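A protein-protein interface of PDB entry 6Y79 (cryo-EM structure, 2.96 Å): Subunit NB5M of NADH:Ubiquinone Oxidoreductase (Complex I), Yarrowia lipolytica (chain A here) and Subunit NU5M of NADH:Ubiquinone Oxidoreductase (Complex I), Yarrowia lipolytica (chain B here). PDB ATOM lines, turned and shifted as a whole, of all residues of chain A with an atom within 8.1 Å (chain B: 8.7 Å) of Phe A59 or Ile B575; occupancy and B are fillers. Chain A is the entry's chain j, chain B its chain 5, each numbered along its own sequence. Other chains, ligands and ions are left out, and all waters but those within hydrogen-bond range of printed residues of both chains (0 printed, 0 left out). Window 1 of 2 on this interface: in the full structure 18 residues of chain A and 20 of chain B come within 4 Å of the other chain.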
ATOM      1  N   ALA A  51      -8.828  30.011   2.374  1.00  0.00           N
ATOM      2  CA  ALA A  51      -9.128  28.681   1.848  1.00  0.00           C
ATOM      3  C   ALA A  51      -8.952  27.621   2.921  1.00  0.00           C
ATOM      4  O   ALA A  51      -9.757  26.682   3.024  1.00  0.00           O
ATOM      5  CB  ALA A  51      -8.229  28.380   0.653  1.00  0.00           C
ATOM      6  N   THR A  52      -7.905  27.773   3.730  1.00  0.00           N
ATOM      7  CA  THR A  52      -7.702  26.929   4.897  1.00  0.00           C
ATOM      8  C   THR A  52      -8.865  27.029   5.875  1.00  0.00           C
ATOM      9  O   THR A  52      -9.359  26.009   6.363  1.00  0.00           O
ATOM     10  CB  THR A  52      -6.396  27.328   5.563  1.00  0.00           C
ATOM     11  OG1 THR A  52      -5.297  26.893   4.755  1.00  0.00           O
ATOM     12  CG2 THR A  52      -6.299  26.731   6.918  1.00  0.00           C
ATOM     13  N   GLY A  53      -9.329  28.246   6.153  1.00  0.00           N
ATOM     14  CA  GLY A  53     -10.431  28.412   7.084  1.00  0.00           C
ATOM     15  C   GLY A  53     -11.738  27.850   6.566  1.00  0.00           C
ATOM     16  O   GLY A  53     -12.521  27.276   7.331  1.00  0.00           O
ATOM     17  N   LYS A  54     -11.980  28.000   5.261  1.00  0.00           N
ATOM     18  CA  LYS A  54     -13.131  27.381   4.618  1.00  0.00           C
ATOM     19  C   LYS A  54     -13.096  25.870   4.772  1.00  0.00           C
ATOM     20  O   LYS A  54     -14.076  25.264   5.212  1.00  0.00           O
ATOM     21  CB  LYS A  54     -13.166  27.770   3.143  1.00  0.00           C
ATOM     22  CG  LYS A  54     -14.364  27.237   2.393  1.00  0.00           C
ATOM     23  CD  LYS A  54     -14.326  27.684   0.949  1.00  0.00           C
ATOM     24  CE  LYS A  54     -13.227  26.965   0.188  1.00  0.00           C
ATOM     25  NZ  LYS A  54     -13.520  25.511   0.052  1.00  0.00           N
ATOM     26  N   SER A  55     -11.945  25.256   4.473  1.00  0.00           N
ATOM     27  CA  SER A  55     -11.811  23.804   4.581  1.00  0.00           C
ATOM     28  C   SER A  55     -11.935  23.326   6.022  1.00  0.00           C
ATOM     29  O   SER A  55     -12.578  22.303   6.289  1.00  0.00           O
ATOM     30  CB  SER A  55     -10.473  23.370   3.995  1.00  0.00           C
ATOM     31  OG  SER A  55     -10.408  23.707   2.626  1.00  0.00           O
ATOM     32  N   THR A  56     -11.359  24.074   6.962  1.00  0.00           N
ATOM     33  CA  THR A  56     -11.356  23.674   8.363  1.00  0.00           C
ATOM     34  C   THR A  56     -12.758  23.733   8.954  1.00  0.00           C
ATOM     35  O   THR A  56     -13.194  22.798   9.635  1.00  0.00           O
ATOM     36  CB  THR A  56     -10.389  24.564   9.144  1.00  0.00           C
ATOM     37  OG1 THR A  56      -9.050  24.302   8.711  1.00  0.00           O
ATOM     38  CG2 THR A  56     -10.489  24.316  10.634  1.00  0.00           C
ATOM     39  N   LEU A  57     -13.499  24.805   8.671  1.00  0.00           N
ATOM     40  CA  LEU A  57     -14.862  24.898   9.179  1.00  0.00           C
ATOM     41  C   LEU A  57     -15.800  23.930   8.470  1.00  0.00           C
ATOM     42  O   LEU A  57     -16.704  23.371   9.095  1.00  0.00           O
ATOM     43  CB  LEU A  57     -15.379  26.330   9.060  1.00  0.00           C
ATOM     44  CG  LEU A  57     -14.751  27.362   9.992  1.00  0.00           C
ATOM     45  CD1 LEU A  57     -15.342  28.723   9.711  1.00  0.00           C
ATOM     46  CD2 LEU A  57     -14.939  26.989  11.455  1.00  0.00           C
ATOM     47  N   ILE A  58     -15.604  23.715   7.167  1.00  0.00           N
ATOM     48  CA  ILE A  58     -16.497  22.824   6.436  1.00  0.00           C
ATOM     49  C   ILE A  58     -16.306  21.368   6.856  1.00  0.00           C
ATOM     50  O   ILE A  58     -17.290  20.649   7.056  1.00  0.00           O
ATOM     51  CB  ILE A  58     -16.309  23.032   4.921  1.00  0.00           C
ATOM     52  CG1 ILE A  58     -17.042  24.293   4.462  1.00  0.00           C
ATOM     53  CG2 ILE A  58     -16.815  21.858   4.110  1.00  0.00           C
ATOM     54  CD1 ILE A  58     -18.537  24.243   4.645  1.00  0.00           C
ATOM     55  N   PHE A  59     -15.070  20.920   7.071  1.00  0.00           N
ATOM     56  CA  PHE A  59     -14.857  19.507   7.351  1.00  0.00           C
ATOM     57  C   PHE A  59     -14.710  19.176   8.828  1.00  0.00           C
ATOM     58  O   PHE A  59     -14.956  18.028   9.206  1.00  0.00           O
ATOM     59  CB  PHE A  59     -13.635  18.999   6.582  1.00  0.00           C
ATOM     60  CG  PHE A  59     -13.845  18.977   5.106  1.00  0.00           C
ATOM     61  CD1 PHE A  59     -14.767  18.109   4.552  1.00  0.00           C
ATOM     62  CD2 PHE A  59     -13.158  19.844   4.275  1.00  0.00           C
ATOM     63  CE1 PHE A  59     -14.996  18.097   3.202  1.00  0.00           C
ATOM     64  CE2 PHE A  59     -13.379  19.832   2.917  1.00  0.00           C
ATOM     65  CZ  PHE A  59     -14.296  18.955   2.381  1.00  0.00           C
ATOM     66  N   LEU A  60     -14.335  20.130   9.677  1.00  0.00           N
ATOM     67  CA  LEU A  60     -14.168  19.827  11.090  1.00  0.00           C
ATOM     68  C   LEU A  60     -15.359  20.211  11.952  1.00  0.00           C
ATOM     69  O   LEU A  60     -15.535  19.609  13.014  1.00  0.00           O
ATOM     70  CB  LEU A  60     -12.928  20.525  11.660  1.00  0.00           C
ATOM     71  CG  LEU A  60     -11.533  20.013  11.321  1.00  0.00           C
ATOM     72  CD1 LEU A  60     -10.525  20.796  12.120  1.00  0.00           C
ATOM     73  CD2 LEU A  60     -11.403  18.556  11.628  1.00  0.00           C
ATOM     74  N   VAL A  61     -16.144  21.227  11.578  1.00  0.00           N
ATOM     75  CA  VAL A  61     -17.274  21.601  12.424  1.00  0.00           C
ATOM     76  C   VAL A  61     -18.606  21.475  11.682  1.00  0.00           C
ATOM     77  O   VAL A  61     -19.605  21.083  12.288  1.00  0.00           O
ATOM     78  CB  VAL A  61     -17.093  23.000  13.078  1.00  0.00           C
ATOM     79  CG1 VAL A  61     -15.722  23.144  13.728  1.00  0.00           C
ATOM     80  CG2 VAL A  61     -17.341  24.173  12.153  1.00  0.00           C
ATOM     81  N   ALA A  62     -18.654  21.781  10.382  1.00  0.00           N
ATOM     82  CA  ALA A  62     -19.949  21.864   9.704  1.00  0.00           C
ATOM     83  C   ALA A  62     -20.501  20.482   9.380  1.00  0.00           C
ATOM     84  O   ALA A  62     -21.658  20.176   9.686  1.00  0.00           O
ATOM     85  CB  ALA A  62     -19.833  22.706   8.435  1.00  0.00           C
ATOM     86  N   PHE A  63     -19.693  19.644   8.758  1.00  0.00           N
ATOM     87  CA  PHE A  63     -20.031  18.260   8.443  1.00  0.00           C
ATOM     88  C   PHE A  63     -20.222  17.370   9.682  1.00  0.00           C
ATOM     89  O   PHE A  63     -21.159  16.551   9.675  1.00  0.00           O
ATOM     90  CB  PHE A  63     -18.969  17.703   7.487  1.00  0.00           C
ATOM     91  CG  PHE A  63     -19.215  16.301   7.050  1.00  0.00           C
ATOM     92  CD1 PHE A  63     -20.170  16.024   6.090  1.00  0.00           C
ATOM     93  CD2 PHE A  63     -18.470  15.259   7.575  1.00  0.00           C
ATOM     94  CE1 PHE A  63     -20.395  14.722   5.675  1.00  0.00           C
ATOM     95  CE2 PHE A  63     -18.690  13.958   7.167  1.00  0.00           C
ATOM     96  CZ  PHE A  63     -19.651  13.690   6.213  1.00  0.00           C
ATOM     97  N   PRO A  64     -19.404  17.475  10.761  1.00  0.00           N
ATOM     98  CA  PRO A  64     -19.788  16.779  12.002  1.00  0.00           C
ATOM     99  C   PRO A  64     -21.103  17.235  12.598  1.00  0.00           C
ATOM    100  O   PRO A  64     -21.869  16.389  13.059  1.00  0.00           O
ATOM    101  CB  PRO A  64     -18.624  17.085  12.945  1.00  0.00           C
ATOM    102  CG  PRO A  64     -17.507  17.222  12.080  1.00  0.00           C
ATOM    103  CD  PRO A  64     -18.007  17.943  10.891  1.00  0.00           C
ATOM    104  N   ALA A  65     -21.401  18.537  12.580  1.00  0.00           N
ATOM    105  CA  ALA A  65     -22.674  19.011  13.115  1.00  0.00           C
ATOM    106  C   ALA A  65     -23.844  18.541  12.264  1.00  0.00           C
ATOM    107  O   ALA A  65     -24.905  18.203  12.799  1.00  0.00           O
ATOM    108  CB  ALA A  65     -22.673  20.533  13.224  1.00  0.00           C
ATOM    109  N   LYS B 567     -13.271  17.915  -9.370  1.00  0.00           N
ATOM    110  CA  LYS B 567     -13.787  18.543  -8.159  1.00  0.00           C
ATOM    111  C   LYS B 567     -13.517  17.682  -6.934  1.00  0.00           C
ATOM    112  O   LYS B 567     -13.075  18.198  -5.901  1.00  0.00           O
ATOM    113  CB  LYS B 567     -15.291  18.794  -8.305  1.00  0.00           C
ATOM    114  CG  LYS B 567     -15.936  19.473  -7.114  1.00  0.00           C
ATOM    115  CD  LYS B 567     -15.417  20.888  -6.919  1.00  0.00           C
ATOM    116  CE  LYS B 567     -15.914  21.835  -8.002  1.00  0.00           C
ATOM    117  NZ  LYS B 567     -15.474  23.239  -7.750  1.00  0.00           N
ATOM    118  N   GLY B 568     -13.739  16.372  -7.049  1.00  0.00           N
ATOM    119  CA  GLY B 568     -13.491  15.480  -5.933  1.00  0.00           C
ATOM    120  C   GLY B 568     -12.027  15.356  -5.582  1.00  0.00           C
ATOM    121  O   GLY B 568     -11.680  15.259  -4.408  1.00  0.00           O
ATOM    122  N   LEU B 569     -11.151  15.380  -6.586  1.00  0.00           N
ATOM    123  CA  LEU B 569      -9.718  15.365  -6.313  1.00  0.00           C
ATOM    124  C   LEU B 569      -9.260  16.658  -5.650  1.00  0.00           C
ATOM    125  O   LEU B 569      -8.379  16.641  -4.784  1.00  0.00           O
ATOM    126  CB  LEU B 569      -8.937  15.125  -7.598  1.00  0.00           C
ATOM    127  CG  LEU B 569      -8.977  13.708  -8.150  1.00  0.00           C
ATOM    128  CD1 LEU B 569      -8.348  13.670  -9.518  1.00  0.00           C
ATOM    129  CD2 LEU B 569      -8.255  12.785  -7.214  1.00  0.00           C
ATOM    130  N   VAL B 570      -9.871  17.786  -6.011  1.00  0.00           N
ATOM    131  CA  VAL B 570      -9.504  19.048  -5.378  1.00  0.00           C
ATOM    132  C   VAL B 570      -9.998  19.104  -3.929  1.00  0.00           C
ATOM    133  O   VAL B 570      -9.259  19.537  -3.037  1.00  0.00           O
ATOM    134  CB  VAL B 570     -10.011  20.223  -6.232  1.00  0.00           C
ATOM    135  CG1 VAL B 570      -9.942  21.525  -5.472  1.00  0.00           C
ATOM    136  CG2 VAL B 570      -9.171  20.331  -7.478  1.00  0.00           C
ATOM    137  N   THR B 571     -11.218  18.616  -3.652  1.00  0.00           N
ATOM    138  CA  THR B 571     -11.662  18.563  -2.255  1.00  0.00           C
ATOM    139  C   THR B 571     -10.879  17.541  -1.438  1.00  0.00           C
ATOM    140  O   THR B 571     -10.655  17.752  -0.243  1.00  0.00           O
ATOM    141  CB  THR B 571     -13.151  18.241  -2.121  1.00  0.00           C
ATOM    142  OG1 THR B 571     -13.383  16.868  -2.458  1.00  0.00           O
ATOM    143  CG2 THR B 571     -14.029  19.168  -2.955  1.00  0.00           C
ATOM    144  N   SER B 572     -10.441  16.442  -2.054  1.00  0.00           N
ATOM    145  CA  SER B 572      -9.637  15.470  -1.324  1.00  0.00           C
ATOM    146  C   SER B 572      -8.255  16.019  -1.020  1.00  0.00           C
ATOM    147  O   SER B 572      -7.682  15.714   0.027  1.00  0.00           O
ATOM    148  CB  SER B 572      -9.536  14.174  -2.118  1.00  0.00           C
ATOM    149  OG  SER B 572      -8.742  14.331  -3.268  1.00  0.00           O
ATOM    150  N   GLY B 573      -7.707  16.842  -1.915  1.00  0.00           N
ATOM    151  CA  GLY B 573      -6.481  17.547  -1.590  1.00  0.00           C
ATOM    152  C   GLY B 573      -6.672  18.601  -0.523  1.00  0.00           C
ATOM    153  O   GLY B 573      -5.771  18.828   0.292  1.00  0.00           O
ATOM    154  N   ASN B 574      -7.843  19.247  -0.507  1.00  0.00           N
ATOM    155  CA  ASN B 574      -8.196  20.161   0.575  1.00  0.00           C
ATOM    156  C   ASN B 574      -8.201  19.452   1.919  1.00  0.00           C
ATOM    157  O   ASN B 574      -7.729  20.006   2.912  1.00  0.00           O
ATOM    158  CB  ASN B 574      -9.565  20.789   0.323  1.00  0.00           C
ATOM    159  CG  ASN B 574      -9.530  21.860  -0.727  1.00  0.00           C
ATOM    160  OD1 ASN B 574      -8.519  22.531  -0.906  1.00  0.00           O
ATOM    161  ND2 ASN B 574     -10.640  22.035  -1.428  1.00  0.00           N
ATOM    162  N   ILE B 575      -8.727  18.230   1.969  1.00  0.00           N
ATOM    163  CA  ILE B 575      -8.750  17.483   3.224  1.00  0.00           C
ATOM    164  C   ILE B 575      -7.354  16.996   3.592  1.00  0.00           C
ATOM    165  O   ILE B 575      -6.910  17.150   4.734  1.00  0.00           O
ATOM    166  CB  ILE B 575      -9.754  16.326   3.141  1.00  0.00           C
ATOM    167  CG1 ILE B 575     -11.160  16.895   3.019  1.00  0.00           C
ATOM    168  CG2 ILE B 575      -9.641  15.430   4.346  1.00  0.00           C
ATOM    169  CD1 ILE B 575     -12.215  15.872   3.099  1.00  0.00           C
ATOM    170  N   ALA B 576      -6.626  16.442   2.622  1.00  0.00           N
ATOM    171  CA  ALA B 576      -5.314  15.876   2.891  1.00  0.00           C
ATOM    172  C   ALA B 576      -4.273  16.927   3.242  1.00  0.00           C
ATOM    173  O   ALA B 576      -3.268  16.590   3.874  1.00  0.00           O
ATOM    174  CB  ALA B 576      -4.846  15.068   1.687  1.00  0.00           C
ATOM    175  N   HIS B 577      -4.482  18.188   2.874  1.00  0.00           N
ATOM    176  CA  HIS B 577      -3.538  19.235   3.226  1.00  0.00           C
ATOM    177  C   HIS B 577      -4.056  20.178   4.298  1.00  0.00           C
ATOM    178  O   HIS B 577      -3.363  20.428   5.282  1.00  0.00           O
ATOM    179  CB  HIS B 577      -3.167  20.042   1.980  1.00  0.00           C
ATOM    180  CG  HIS B 577      -2.455  19.248   0.937  1.00  0.00           C
ATOM    181  ND1 HIS B 577      -3.120  18.540  -0.040  1.00  0.00           N
ATOM    182  CD2 HIS B 577      -1.136  19.053   0.711  1.00  0.00           C
ATOM    183  CE1 HIS B 577      -2.242  17.941  -0.821  1.00  0.00           C
ATOM    184  NE2 HIS B 577      -1.031  18.238  -0.388  1.00  0.00           N
ATOM    185  N   HIS B 578      -5.254  20.729   4.128  1.00  0.00           N
ATOM    186  CA  HIS B 578      -5.742  21.775   5.012  1.00  0.00           C
ATOM    187  C   HIS B 578      -6.374  21.238   6.282  1.00  0.00           C
ATOM    188  O   HIS B 578      -6.451  21.970   7.271  1.00  0.00           O
ATOM    189  CB  HIS B 578      -6.753  22.653   4.277  1.00  0.00           C
ATOM    190  CG  HIS B 578      -6.195  23.311   3.060  1.00  0.00           C
ATOM    191  ND1 HIS B 578      -5.208  24.268   3.125  1.00  0.00           N
ATOM    192  CD2 HIS B 578      -6.476  23.147   1.749  1.00  0.00           C
ATOM    193  CE1 HIS B 578      -4.904  24.665   1.903  1.00  0.00           C
ATOM    194  NE2 HIS B 578      -5.658  23.999   1.050  1.00  0.00           N
ATOM    195  N   VAL B 579      -6.838  19.998   6.284  1.00  0.00           N
ATOM    196  CA  VAL B 579      -7.493  19.407   7.444  1.00  0.00           C
ATOM    197  C   VAL B 579      -6.582  18.408   8.142  1.00  0.00           C
ATOM    198  O   VAL B 579      -6.308  18.536   9.333  1.00  0.00           O
ATOM    199  CB  VAL B 579      -8.841  18.763   7.055  1.00  0.00           C
ATOM    200  CG1 VAL B 579      -9.449  18.058   8.241  1.00  0.00           C
ATOM    201  CG2 VAL B 579      -9.782  19.810   6.536  1.00  0.00           C
ATOM    202  N   ASP B 580      -6.081  17.415   7.409  1.00  0.00           N
ATOM    203  CA  ASP B 580      -5.355  16.324   8.048  1.00  0.00           C
ATOM    204  C   ASP B 580      -3.918  16.707   8.348  1.00  0.00           C
ATOM    205  O   ASP B 580      -3.438  16.487   9.456  1.00  0.00           O
ATOM    206  CB  ASP B 580      -5.417  15.067   7.187  1.00  0.00           C
ATOM    207  CG  ASP B 580      -6.791  14.428   7.204  1.00  0.00           C
ATOM    208  OD1 ASP B 580      -7.773  15.139   7.512  1.00  0.00           O
ATOM    209  OD2 ASP B 580      -6.893  13.215   6.923  1.00  0.00           O
ATOM    210  N   LYS B 581      -3.208  17.272   7.380  1.00  0.00           N
ATOM    211  CA  LYS B 581      -1.878  17.788   7.664  1.00  0.00           C
ATOM    212  C   LYS B 581      -1.891  19.231   8.123  1.00  0.00           C
ATOM    213  O   LYS B 581      -0.862  19.727   8.583  1.00  0.00           O
ATOM    214  CB  LYS B 581      -0.975  17.659   6.441  1.00  0.00           C
ATOM    215  CG  LYS B 581      -0.448  16.265   6.254  1.00  0.00           C
ATOM    216  CD  LYS B 581       0.472  16.163   5.073  1.00  0.00           C
ATOM    217  CE  LYS B 581       0.840  14.717   4.820  1.00  0.00           C
ATOM    218  NZ  LYS B 581       1.644  14.548   3.586  1.00  0.00           N
ATOM    219  N   GLY B 582      -3.002  19.926   7.972  1.00  0.00           N
ATOM    220  CA  GLY B 582      -3.046  21.293   8.418  1.00  0.00           C
ATOM    221  C   GLY B 582      -3.544  21.585   9.812  1.00  0.00           C
ATOM    222  O   GLY B 582      -2.801  22.108  10.642  1.00  0.00           O
ATOM    223  N   SER B 583      -4.794  21.250  10.095  1.00  0.00           N
ATOM    224  CA  SER B 583      -5.415  21.711  11.324  1.00  0.00           C
ATOM    225  C   SER B 583      -5.534  20.625  12.375  1.00  0.00           C
ATOM    226  O   SER B 583      -5.745  20.942  13.548  1.00  0.00           O
ATOM    227  CB  SER B 583      -6.800  22.292  11.040  1.00  0.00           C
ATOM    228  OG  SER B 583      -7.666  21.292  10.555  1.00  0.00           O
ATOM    229  N   LEU B 584      -5.416  19.361  11.988  1.00  0.00           N
ATOM    230  CA  LEU B 584      -5.313  18.291  12.965  1.00  0.00           C
ATOM    231  C   LEU B 584      -3.895  18.124  13.487  1.00  0.00           C
ATOM    232  O   LEU B 584      -3.680  17.324  14.400  1.00  0.00           O
ATOM    233  CB  LEU B 584      -5.796  16.977  12.369  1.00  0.00           C
ATOM    234  CG  LEU B 584      -7.295  16.947  12.095  1.00  0.00           C
ATOM    235  CD1 LEU B 584      -7.665  15.707  11.340  1.00  0.00           C
ATOM    236  CD2 LEU B 584      -8.065  17.033  13.382  1.00  0.00           C
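Of the 18 printed residues of chain B, 5 touch a printed residue of chain A.
Printed residues of chain B that touch a printed residue of chain A: Asn B574, Ile B575, His B578, Val B579 and Ser B583.
Hydrophobic or aromatic side chains of chain B that line the printed part of chain A: Ile B575, His B578 and Val B579.
Among the printed residues, no Asp or Glu carboxylate lies within 4 Å of a Lys or Arg side-chain nitrogen of the other chain.
The side-chain hydroxyl (OG1) of Thr A52 sits at hydrogen-bond distance from a ring nitrogen (ND1) of His B578, at 3.1 Å.
Asn B574 touches Ser A55 (CB to OG, 3.8 Å).
CB of Ser A55 touches CB of His B578 (3.8 Å).
O of Ser A55 touches CG2 of Val B579, at 3.8 Å.
OG1 of Thr A56 touches O of His B578 (3.8 Å).
Thr A56 touches Ser B583.
CE1 of Phe A59 touches CD1 of Ile B575, at 3.6 Å.
CB of Phe A59 touches CG2 of Val B579, at 3.9 Å.
CD2 of Leu A60 touches CG1 of Val B579, at 3.9 Å.
Ser B583 touches Leu A60.
Printed residues of chain B within 4 Å of Phe A59: Ile B575 (3.6 Å) and Val B579 (3.9 Å).
Ile B575 touches just one residue of chain A: Phe A59.
No residue of chain A comes within 4 Å of Ala B576.
Of the printed residues of chain A, Ser B583 touches Thr A56 (3.8 Å) and Leu A60 (3.3 Å).
Of the printed residues of chain B, Thr A52 touches His B578.
Printed residues of chain B within 4 Å of Leu A60: Val B579 (3.9 Å) and Ser B583 (3.3 Å).
Printed residues of chain A within 4 Å of Val B579: Ser A55 (3.8 Å), Phe A59 (3.9 Å) and Leu A60 (3.9 Å).
Printed residues of chain A within 4 Å of Asn B574: Ser A55.
Ser B572 touches none of the printed residues of chain A.
The nearest residue of chain B that does not touch Phe A59 is Thr B571 (4.6 Å).
The nearest residue of chain A that does not touch Ile B575 is Ser A55 (5.8 Å).
The nearest printed residue of chain B that does not touch Ser A55 is Ile B575 (5.8 Å).
The backbone carbonyl oxygen (O) of His B578 is in hydrogen-bond range of the backbone NH (N) of Ser B583 (3.4 Å).
The backbone carbonyl oxygen of Ile B575 lies within hydrogen-bond range of the backbone NH of Asp B580 (2.8 Å).
O of Val B570 lies within hydrogen-bond range of ND2 of Asn B574 (3.3 Å).
The backbone carbonyl oxygen (O) of Val B579 sits at hydrogen-bond distance from the side-chain hydroxyl (OG) of Ser B583 (3.3 Å).
The backbone carbonyl oxygen (O) of Thr A52 sits at hydrogen-bond distance from the side-chain hydroxyl (OG1) of Thr A56 (2.9 Å).
The backbone NH (N) of Val B579 is in hydrogen-bond range of the backbone carbonyl oxygen (O) of Asn B574.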
